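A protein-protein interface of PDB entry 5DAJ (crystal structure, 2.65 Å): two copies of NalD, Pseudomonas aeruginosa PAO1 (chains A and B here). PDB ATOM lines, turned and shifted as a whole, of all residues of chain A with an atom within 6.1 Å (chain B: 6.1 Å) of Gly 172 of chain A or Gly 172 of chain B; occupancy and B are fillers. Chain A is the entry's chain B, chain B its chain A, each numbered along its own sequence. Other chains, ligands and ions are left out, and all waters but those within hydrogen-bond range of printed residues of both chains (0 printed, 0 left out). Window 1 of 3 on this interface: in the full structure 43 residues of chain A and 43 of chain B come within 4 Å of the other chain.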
ATOM      1  N   HIS A 167     -19.633  26.401 -20.632  1.00  0.00           N
ATOM      2  CA  HIS A 167     -20.035  25.379 -21.593  1.00  0.00           C
ATOM      3  C   HIS A 167     -21.546  25.285 -21.736  1.00  0.00           C
ATOM      4  O   HIS A 167     -22.066  25.136 -22.845  1.00  0.00           O
ATOM      5  CB  HIS A 167     -19.496  23.999 -21.235  1.00  0.00           C
ATOM      6  CG  HIS A 167     -19.927  22.942 -22.204  1.00  0.00           C
ATOM      7  ND1 HIS A 167     -21.011  22.126 -21.978  1.00  0.00           N
ATOM      8  CD2 HIS A 167     -19.473  22.635 -23.440  1.00  0.00           C
ATOM      9  CE1 HIS A 167     -21.185  21.331 -23.018  1.00  0.00           C
ATOM     10  NE2 HIS A 167     -20.261  21.615 -23.918  1.00  0.00           N
ATOM     11  N   ALA A 168     -22.235  25.348 -20.604  1.00  0.00           N
ATOM     12  CA  ALA A 168     -23.693  25.317 -20.585  1.00  0.00           C
ATOM     13  C   ALA A 168     -24.260  26.460 -21.424  1.00  0.00           C
ATOM     14  O   ALA A 168     -25.186  26.252 -22.212  1.00  0.00           O
ATOM     15  CB  ALA A 168     -24.223  25.390 -19.163  1.00  0.00           C
ATOM     16  N   LEU A 169     -23.682  27.648 -21.285  1.00  0.00           N
ATOM     17  CA  LEU A 169     -24.122  28.798 -22.082  1.00  0.00           C
ATOM     18  C   LEU A 169     -23.961  28.555 -23.580  1.00  0.00           C
ATOM     19  O   LEU A 169     -24.895  28.781 -24.347  1.00  0.00           O
ATOM     20  CB  LEU A 169     -23.387  30.082 -21.691  1.00  0.00           C
ATOM     21  CG  LEU A 169     -23.726  31.310 -22.553  1.00  0.00           C
ATOM     22  CD1 LEU A 169     -25.198  31.666 -22.470  1.00  0.00           C
ATOM     23  CD2 LEU A 169     -22.878  32.493 -22.140  1.00  0.00           C
ATOM     24  N   ILE A 170     -22.780  28.094 -23.983  1.00  0.00           N
ATOM     25  CA  ILE A 170     -22.506  27.800 -25.398  1.00  0.00           C
ATOM     26  C   ILE A 170     -23.485  26.758 -25.924  1.00  0.00           C
ATOM     27  O   ILE A 170     -24.083  26.941 -26.988  1.00  0.00           O
ATOM     28  CB  ILE A 170     -21.080  27.272 -25.660  1.00  0.00           C
ATOM     29  CG1 ILE A 170     -20.005  28.219 -25.104  1.00  0.00           C
ATOM     30  CG2 ILE A 170     -20.848  27.078 -27.156  1.00  0.00           C
ATOM     31  CD1 ILE A 170     -20.143  29.669 -25.535  1.00  0.00           C
ATOM     32  N   LEU A 171     -23.629  25.672 -25.176  1.00  0.00           N
ATOM     33  CA  LEU A 171     -24.518  24.580 -25.548  1.00  0.00           C
ATOM     34  C   LEU A 171     -25.955  25.055 -25.686  1.00  0.00           C
ATOM     35  O   LEU A 171     -26.645  24.696 -26.642  1.00  0.00           O
ATOM     36  CB  LEU A 171     -24.467  23.473 -24.505  1.00  0.00           C
ATOM     37  CG  LEU A 171     -25.390  22.269 -24.718  1.00  0.00           C
ATOM     38  CD1 LEU A 171     -25.068  21.536 -26.013  1.00  0.00           C
ATOM     39  CD2 LEU A 171     -25.271  21.334 -23.540  1.00  0.00           C
ATOM     40  N   GLY A 172     -26.387  25.870 -24.729  1.00  0.00           N
ATOM     41  CA  GLY A 172     -27.730  26.445 -24.731  1.00  0.00           C
ATOM     42  C   GLY A 172     -28.010  27.349 -25.918  1.00  0.00           C
ATOM     43  O   GLY A 172     -29.079  27.264 -26.528  1.00  0.00           O
ATOM     44  N   LEU A 173     -27.046  28.203 -26.253  1.00  0.00           N
ATOM     45  CA  LEU A 173     -27.164  29.076 -27.418  1.00  0.00           C
ATOM     46  C   LEU A 173     -27.338  28.271 -28.710  1.00  0.00           C
ATOM     47  O   LEU A 173     -28.201  28.586 -29.537  1.00  0.00           O
ATOM     48  CB  LEU A 173     -25.948  29.994 -27.552  1.00  0.00           C
ATOM     49  CG  LEU A 173     -25.829  31.088 -26.495  1.00  0.00           C
ATOM     50  CD1 LEU A 173     -24.473  31.754 -26.602  1.00  0.00           C
ATOM     51  CD2 LEU A 173     -26.937  32.113 -26.626  1.00  0.00           C
ATOM     52  N   PHE A 174     -26.501  27.256 -28.873  1.00  0.00           N
ATOM     53  CA  PHE A 174     -26.602  26.321 -30.003  1.00  0.00           C
ATOM     54  C   PHE A 174     -27.991  25.679 -30.039  1.00  0.00           C
ATOM     55  O   PHE A 174     -28.657  25.676 -31.075  1.00  0.00           O
ATOM     56  CB  PHE A 174     -25.538  25.214 -29.919  1.00  0.00           C
ATOM     57  CG  PHE A 174     -24.211  25.596 -30.513  1.00  0.00           C
ATOM     58  CD1 PHE A 174     -23.569  26.757 -30.136  1.00  0.00           C
ATOM     59  CD2 PHE A 174     -23.600  24.779 -31.437  1.00  0.00           C
ATOM     60  CE1 PHE A 174     -22.349  27.103 -30.681  1.00  0.00           C
ATOM     61  CE2 PHE A 174     -22.378  25.118 -31.992  1.00  0.00           C
ATOM     62  CZ  PHE A 174     -21.749  26.286 -31.613  1.00  0.00           C
ATOM     63  N   ASN A 175     -28.418  25.172 -28.891  1.00  0.00           N
ATOM     64  CA  ASN A 175     -29.688  24.470 -28.790  1.00  0.00           C
ATOM     65  C   ASN A 175     -30.872  25.369 -29.121  1.00  0.00           C
ATOM     66  O   ASN A 175     -31.724  25.020 -29.935  1.00  0.00           O
ATOM     67  CB  ASN A 175     -29.869  23.893 -27.395  1.00  0.00           C
ATOM     68  CG  ASN A 175     -30.619  22.591 -27.408  1.00  0.00           C
ATOM     69  OD1 ASN A 175     -31.844  22.581 -27.335  1.00  0.00           O
ATOM     70  ND2 ASN A 175     -29.894  21.482 -27.508  1.00  0.00           N
ATOM     71  N   ASP A 176     -30.908  26.532 -28.474  1.00  0.00           N
ATOM     72  CA  ASP A 176     -31.957  27.538 -28.709  1.00  0.00           C
ATOM     73  C   ASP A 176     -32.021  27.948 -30.177  1.00  0.00           C
ATOM     74  O   ASP A 176     -33.093  27.920 -30.783  1.00  0.00           O
ATOM     75  CB  ASP A 176     -31.755  28.794 -27.839  1.00  0.00           C
ATOM     76  CG  ASP A 176     -32.640  28.820 -26.598  1.00  0.00           C
ATOM     77  OD1 ASP A 176     -33.638  28.078 -26.529  1.00  0.00           O
ATOM     78  OD2 ASP A 176     -32.350  29.622 -25.683  1.00  0.00           O
ATOM     79  N   TRP A 177     -30.876  28.328 -30.735  1.00  0.00           N
ATOM     80  CA  TRP A 177     -30.850  28.881 -32.086  1.00  0.00           C
ATOM     81  C   TRP A 177     -31.250  27.848 -33.130  1.00  0.00           C
ATOM     82  O   TRP A 177     -32.002  28.156 -34.050  1.00  0.00           O
ATOM     83  CB  TRP A 177     -29.489  29.472 -32.448  1.00  0.00           C
ATOM     84  CG  TRP A 177     -29.580  30.248 -33.714  1.00  0.00           C
ATOM     85  CD1 TRP A 177     -30.048  31.514 -33.859  1.00  0.00           C
ATOM     86  CD2 TRP A 177     -29.239  29.795 -35.021  1.00  0.00           C
ATOM     87  NE1 TRP A 177     -30.009  31.889 -35.179  1.00  0.00           N
ATOM     88  CE2 TRP A 177     -29.520  30.851 -35.919  1.00  0.00           C
ATOM     89  CE3 TRP A 177     -28.726  28.604 -35.523  1.00  0.00           C
ATOM     90  CZ2 TRP A 177     -29.302  30.756 -37.292  1.00  0.00           C
ATOM     91  CZ3 TRP A 177     -28.512  28.506 -36.892  1.00  0.00           C
ATOM     92  CH2 TRP A 177     -28.803  29.579 -37.760  1.00  0.00           C
ATOM     93  N   HIS B 167     -31.885  32.580 -20.854  1.00  0.00           N
ATOM     94  CA  HIS B 167     -32.604  31.355 -21.188  1.00  0.00           C
ATOM     95  C   HIS B 167     -31.669  30.273 -21.718  1.00  0.00           C
ATOM     96  O   HIS B 167     -31.816  29.094 -21.363  1.00  0.00           O
ATOM     97  CB  HIS B 167     -33.716  31.578 -22.209  1.00  0.00           C
ATOM     98  CG  HIS B 167     -34.439  30.319 -22.564  1.00  0.00           C
ATOM     99  ND1 HIS B 167     -34.133  29.577 -23.682  1.00  0.00           N
ATOM    100  CD2 HIS B 167     -35.385  29.620 -21.897  1.00  0.00           C
ATOM    101  CE1 HIS B 167     -34.889  28.497 -23.709  1.00  0.00           C
ATOM    102  NE2 HIS B 167     -35.661  28.499 -22.636  1.00  0.00           N
ATOM    103  N   ALA B 168     -30.749  30.672 -22.588  1.00  0.00           N
ATOM    104  CA  ALA B 168     -29.759  29.751 -23.138  1.00  0.00           C
ATOM    105  C   ALA B 168     -28.948  29.093 -22.018  1.00  0.00           C
ATOM    106  O   ALA B 168     -28.742  27.883 -22.038  1.00  0.00           O
ATOM    107  CB  ALA B 168     -28.832  30.467 -24.102  1.00  0.00           C
ATOM    108  N   LEU B 169     -28.535  29.880 -21.027  1.00  0.00           N
ATOM    109  CA  LEU B 169     -27.804  29.335 -19.878  1.00  0.00           C
ATOM    110  C   LEU B 169     -28.621  28.296 -19.114  1.00  0.00           C
ATOM    111  O   LEU B 169     -28.129  27.202 -18.842  1.00  0.00           O
ATOM    112  CB  LEU B 169     -27.366  30.426 -18.909  1.00  0.00           C
ATOM    113  CG  LEU B 169     -26.686  29.921 -17.630  1.00  0.00           C
ATOM    114  CD1 LEU B 169     -25.421  29.148 -17.945  1.00  0.00           C
ATOM    115  CD2 LEU B 169     -26.376  31.080 -16.710  1.00  0.00           C
ATOM    116  N   ILE B 170     -29.873  28.631 -18.789  1.00  0.00           N
ATOM    117  CA  ILE B 170     -30.766  27.694 -18.078  1.00  0.00           C
ATOM    118  C   ILE B 170     -30.943  26.405 -18.883  1.00  0.00           C
ATOM    119  O   ILE B 170     -30.810  25.304 -18.349  1.00  0.00           O
ATOM    120  CB  ILE B 170     -32.175  28.265 -17.807  1.00  0.00           C
ATOM    121  CG1 ILE B 170     -32.114  29.598 -17.064  1.00  0.00           C
ATOM    122  CG2 ILE B 170     -33.008  27.275 -17.000  1.00  0.00           C
ATOM    123  CD1 ILE B 170     -31.265  29.589 -15.807  1.00  0.00           C
ATOM    124  N   LEU B 171     -31.257  26.563 -20.163  1.00  0.00           N
ATOM    125  CA  LEU B 171     -31.464  25.433 -21.062  1.00  0.00           C
ATOM    126  C   LEU B 171     -30.227  24.553 -21.134  1.00  0.00           C
ATOM    127  O   LEU B 171     -30.330  23.330 -21.098  1.00  0.00           O
ATOM    128  CB  LEU B 171     -31.816  25.922 -22.462  1.00  0.00           C
ATOM    129  CG  LEU B 171     -32.017  24.862 -23.539  1.00  0.00           C
ATOM    130  CD1 LEU B 171     -33.164  23.925 -23.200  1.00  0.00           C
ATOM    131  CD2 LEU B 171     -32.263  25.533 -24.874  1.00  0.00           C
ATOM    132  N   GLY B 172     -29.069  25.194 -21.250  1.00  0.00           N
ATOM    133  CA  GLY B 172     -27.790  24.502 -21.324  1.00  0.00           C
ATOM    134  C   GLY B 172     -27.462  23.706 -20.073  1.00  0.00           C
ATOM    135  O   GLY B 172     -26.997  22.575 -20.158  1.00  0.00           O
ATOM    136  N   LEU B 173     -27.721  24.297 -18.914  1.00  0.00           N
ATOM    137  CA  LEU B 173     -27.516  23.613 -17.637  1.00  0.00           C
ATOM    138  C   LEU B 173     -28.371  22.350 -17.523  1.00  0.00           C
ATOM    139  O   LEU B 173     -27.876  21.295 -17.129  1.00  0.00           O
ATOM    140  CB  LEU B 173     -27.815  24.543 -16.459  1.00  0.00           C
ATOM    141  CG  LEU B 173     -26.823  25.683 -16.245  1.00  0.00           C
ATOM    142  CD1 LEU B 173     -27.377  26.638 -15.207  1.00  0.00           C
ATOM    143  CD2 LEU B 173     -25.463  25.167 -15.818  1.00  0.00           C
ATOM    144  N   PHE B 174     -29.648  22.484 -17.870  1.00  0.00           N
ATOM    145  CA  PHE B 174     -30.579  21.346 -17.935  1.00  0.00           C
ATOM    146  C   PHE B 174     -30.039  20.279 -18.876  1.00  0.00           C
ATOM    147  O   PHE B 174     -29.949  19.110 -18.522  1.00  0.00           O
ATOM    148  CB  PHE B 174     -31.966  21.782 -18.416  1.00  0.00           C
ATOM    149  CG  PHE B 174     -32.863  22.290 -17.320  1.00  0.00           C
ATOM    150  CD1 PHE B 174     -32.444  23.293 -16.473  1.00  0.00           C
ATOM    151  CD2 PHE B 174     -34.148  21.774 -17.160  1.00  0.00           C
ATOM    152  CE1 PHE B 174     -33.276  23.760 -15.469  1.00  0.00           C
ATOM    153  CE2 PHE B 174     -34.991  22.235 -16.160  1.00  0.00           C
ATOM    154  CZ  PHE B 174     -34.553  23.236 -15.314  1.00  0.00           C
ATOM    155  N   ASN B 175     -29.641  20.709 -20.062  1.00  0.00           N
ATOM    156  CA  ASN B 175     -29.157  19.798 -21.094  1.00  0.00           C
ATOM    157  C   ASN B 175     -27.890  19.055 -20.666  1.00  0.00           C
ATOM    158  O   ASN B 175     -27.820  17.829 -20.762  1.00  0.00           O
ATOM    159  CB  ASN B 175     -28.880  20.547 -22.397  1.00  0.00           C
ATOM    160  CG  ASN B 175     -29.178  19.715 -23.610  1.00  0.00           C
ATOM    161  OD1 ASN B 175     -28.315  18.985 -24.098  1.00  0.00           O
ATOM    162  ND2 ASN B 175     -30.406  19.810 -24.107  1.00  0.00           N
ATOM    163  N   ASP B 176     -26.900  19.820 -20.200  1.00  0.00           N
ATOM    164  CA  ASP B 176     -25.629  19.261 -19.711  1.00  0.00           C
ATOM    165  C   ASP B 176     -25.864  18.265 -18.590  1.00  0.00           C
ATOM    166  O   ASP B 176     -25.366  17.140 -18.640  1.00  0.00           O
ATOM    167  CB  ASP B 176     -24.663  20.359 -19.221  1.00  0.00           C
ATOM    168  CG  ASP B 176     -23.583  20.717 -20.235  1.00  0.00           C
ATOM    169  OD1 ASP B 176     -23.335  19.949 -21.182  1.00  0.00           O
ATOM    170  OD2 ASP B 176     -22.954  21.785 -20.075  1.00  0.00           O
ATOM    171  N   TRP B 177     -26.617  18.680 -17.577  1.00  0.00           N
ATOM    172  CA  TRP B 177     -26.790  17.857 -16.377  1.00  0.00           C
ATOM    173  C   TRP B 177     -27.548  16.570 -16.663  1.00  0.00           C
ATOM    174  O   TRP B 177     -27.168  15.510 -16.183  1.00  0.00           O
ATOM    175  CB  TRP B 177     -27.496  18.603 -15.249  1.00  0.00           C
ATOM    176  CG  TRP B 177     -27.417  17.828 -13.981  1.00  0.00           C
ATOM    177  CD1 TRP B 177     -26.352  17.769 -13.136  1.00  0.00           C
ATOM    178  CD2 TRP B 177     -28.411  16.969 -13.437  1.00  0.00           C
ATOM    179  NE1 TRP B 177     -26.629  16.935 -12.088  1.00  0.00           N
ATOM    180  CE2 TRP B 177     -27.888  16.428 -12.247  1.00  0.00           C
ATOM    181  CE3 TRP B 177     -29.699  16.605 -13.831  1.00  0.00           C
ATOM    182  CZ2 TRP B 177     -28.609  15.541 -11.441  1.00  0.00           C
ATOM    183  CZ3 TRP B 177     -30.418  15.720 -13.029  1.00  0.00           C
ATOM    184  CH2 TRP B 177     -29.870  15.200 -11.849  1.00  0.00           C
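ND1 of His 167 of chain A is in hydrogen-bond range of OD2 of Asp 176 of chain B (2.7 Å). A ring nitrogen (ND1) of His 167 of chain B sits at hydrogen-bond distance from the side-chain carboxylate (OD2) of Asp 176 of chain A, at 2.7 Å.
Printed residues of chain B within 4 Å of Gly 172 of chain A: Ala 168 (3.2 Å), Leu 171 (3.98 Å) and Gly 172 (3.9 Å). Of the printed residues of chain A, Gly 172 of chain B touches Ala 168 (3.3 Å), Leu 171 (3.99 Å) and Gly 172 (3.9 Å). Printed residues of chain A within 4 Å of Ala 168 of chain B: Ala 168 (3.9 Å), Gly 172 (3.2 Å), Leu 173 (3.6 Å) and Asp 176 (3.6 Å). Of the printed residues of chain B, Leu 171 of chain A touches Gly 172 (3.99 Å), Asn 175 (3.9 Å) and Asp 176 (3.4 Å). Printed residues of chain A within 4 Å of Asn 175 of chain B: Leu 171 and Asn 175. Ile 170 of chain B touches none of the printed residues of chain A. Leu 169 of chain A touches none of the printed residues of chain B.
Of the 11 printed residues of chain A, 7 touch a printed residue of chain B. Printed residues of chain A that touch a printed residue of chain B: His 167, Ala 168, Leu 171, Gly 172, Leu 173, Asn 175 and Asp 176. Hydrophobic or aromatic side chains of chain A within 4 Å of the printed part of chain B: His 167, Ala 168, Leu 171 and Leu 173. Among the printed residues, 17 pairs touch across the chains. Among the printed residues, no Asp or Glu carboxylate lies within 4 Å of a Lys or Arg side-chain nitrogen of the other chain.
Among the printed residues, merely in contact across the chains: Gly 172 of chain A with Ala 168 of chain B, Ala 168 of chain A with Gly 172 of chain B, Asp 176 of chain A with Leu 171 of chain B, Leu 171 of chain A with Asp 176 of chain B, Leu 173 of chain A with Ala 168 of chain B, Ala 168 of chain A with Leu 173 of chain B, Asp 176 of chain A with Ala 168 of chain B, Ala 168 of chain A with Asp 176 of chain B, Asn 175 of chain A with Asn 175 of chain B, Asn 175 of chain A with Leu 171 of chain B, Leu 171 of chain A with Asn 175 of chain B, Ala 168 of chain A with Ala 168 of chain B, Gly 172 of chain A with Gly 172 of chain B, Gly 172 of chain A with Leu 171 of chain B and Leu 171 of chain A with Gly 172 of chain B.
Ala 168 of chain A touches Gly 172 of chain B, and with the chains exchanged Gly 172 of chain A touches Ala 168 of chain B. Leu 171 of chain A touches Gly 172 of chain B, and with the chains exchanged Gly 172 of chain A touches Leu 171 of chain B. Leu 171 of chain A touches Asp 176 of chain B, and with the chains exchanged Asp 176 of chain A touches Leu 171 of chain B. Asn 175 of chain A touches its own counterpart, Asn 175 of chain B. 11 positions are printed for both chains. Of the 17 pairs that touch across the chains among the printed residues, 17 have their exchanged pair printed and touching as well.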
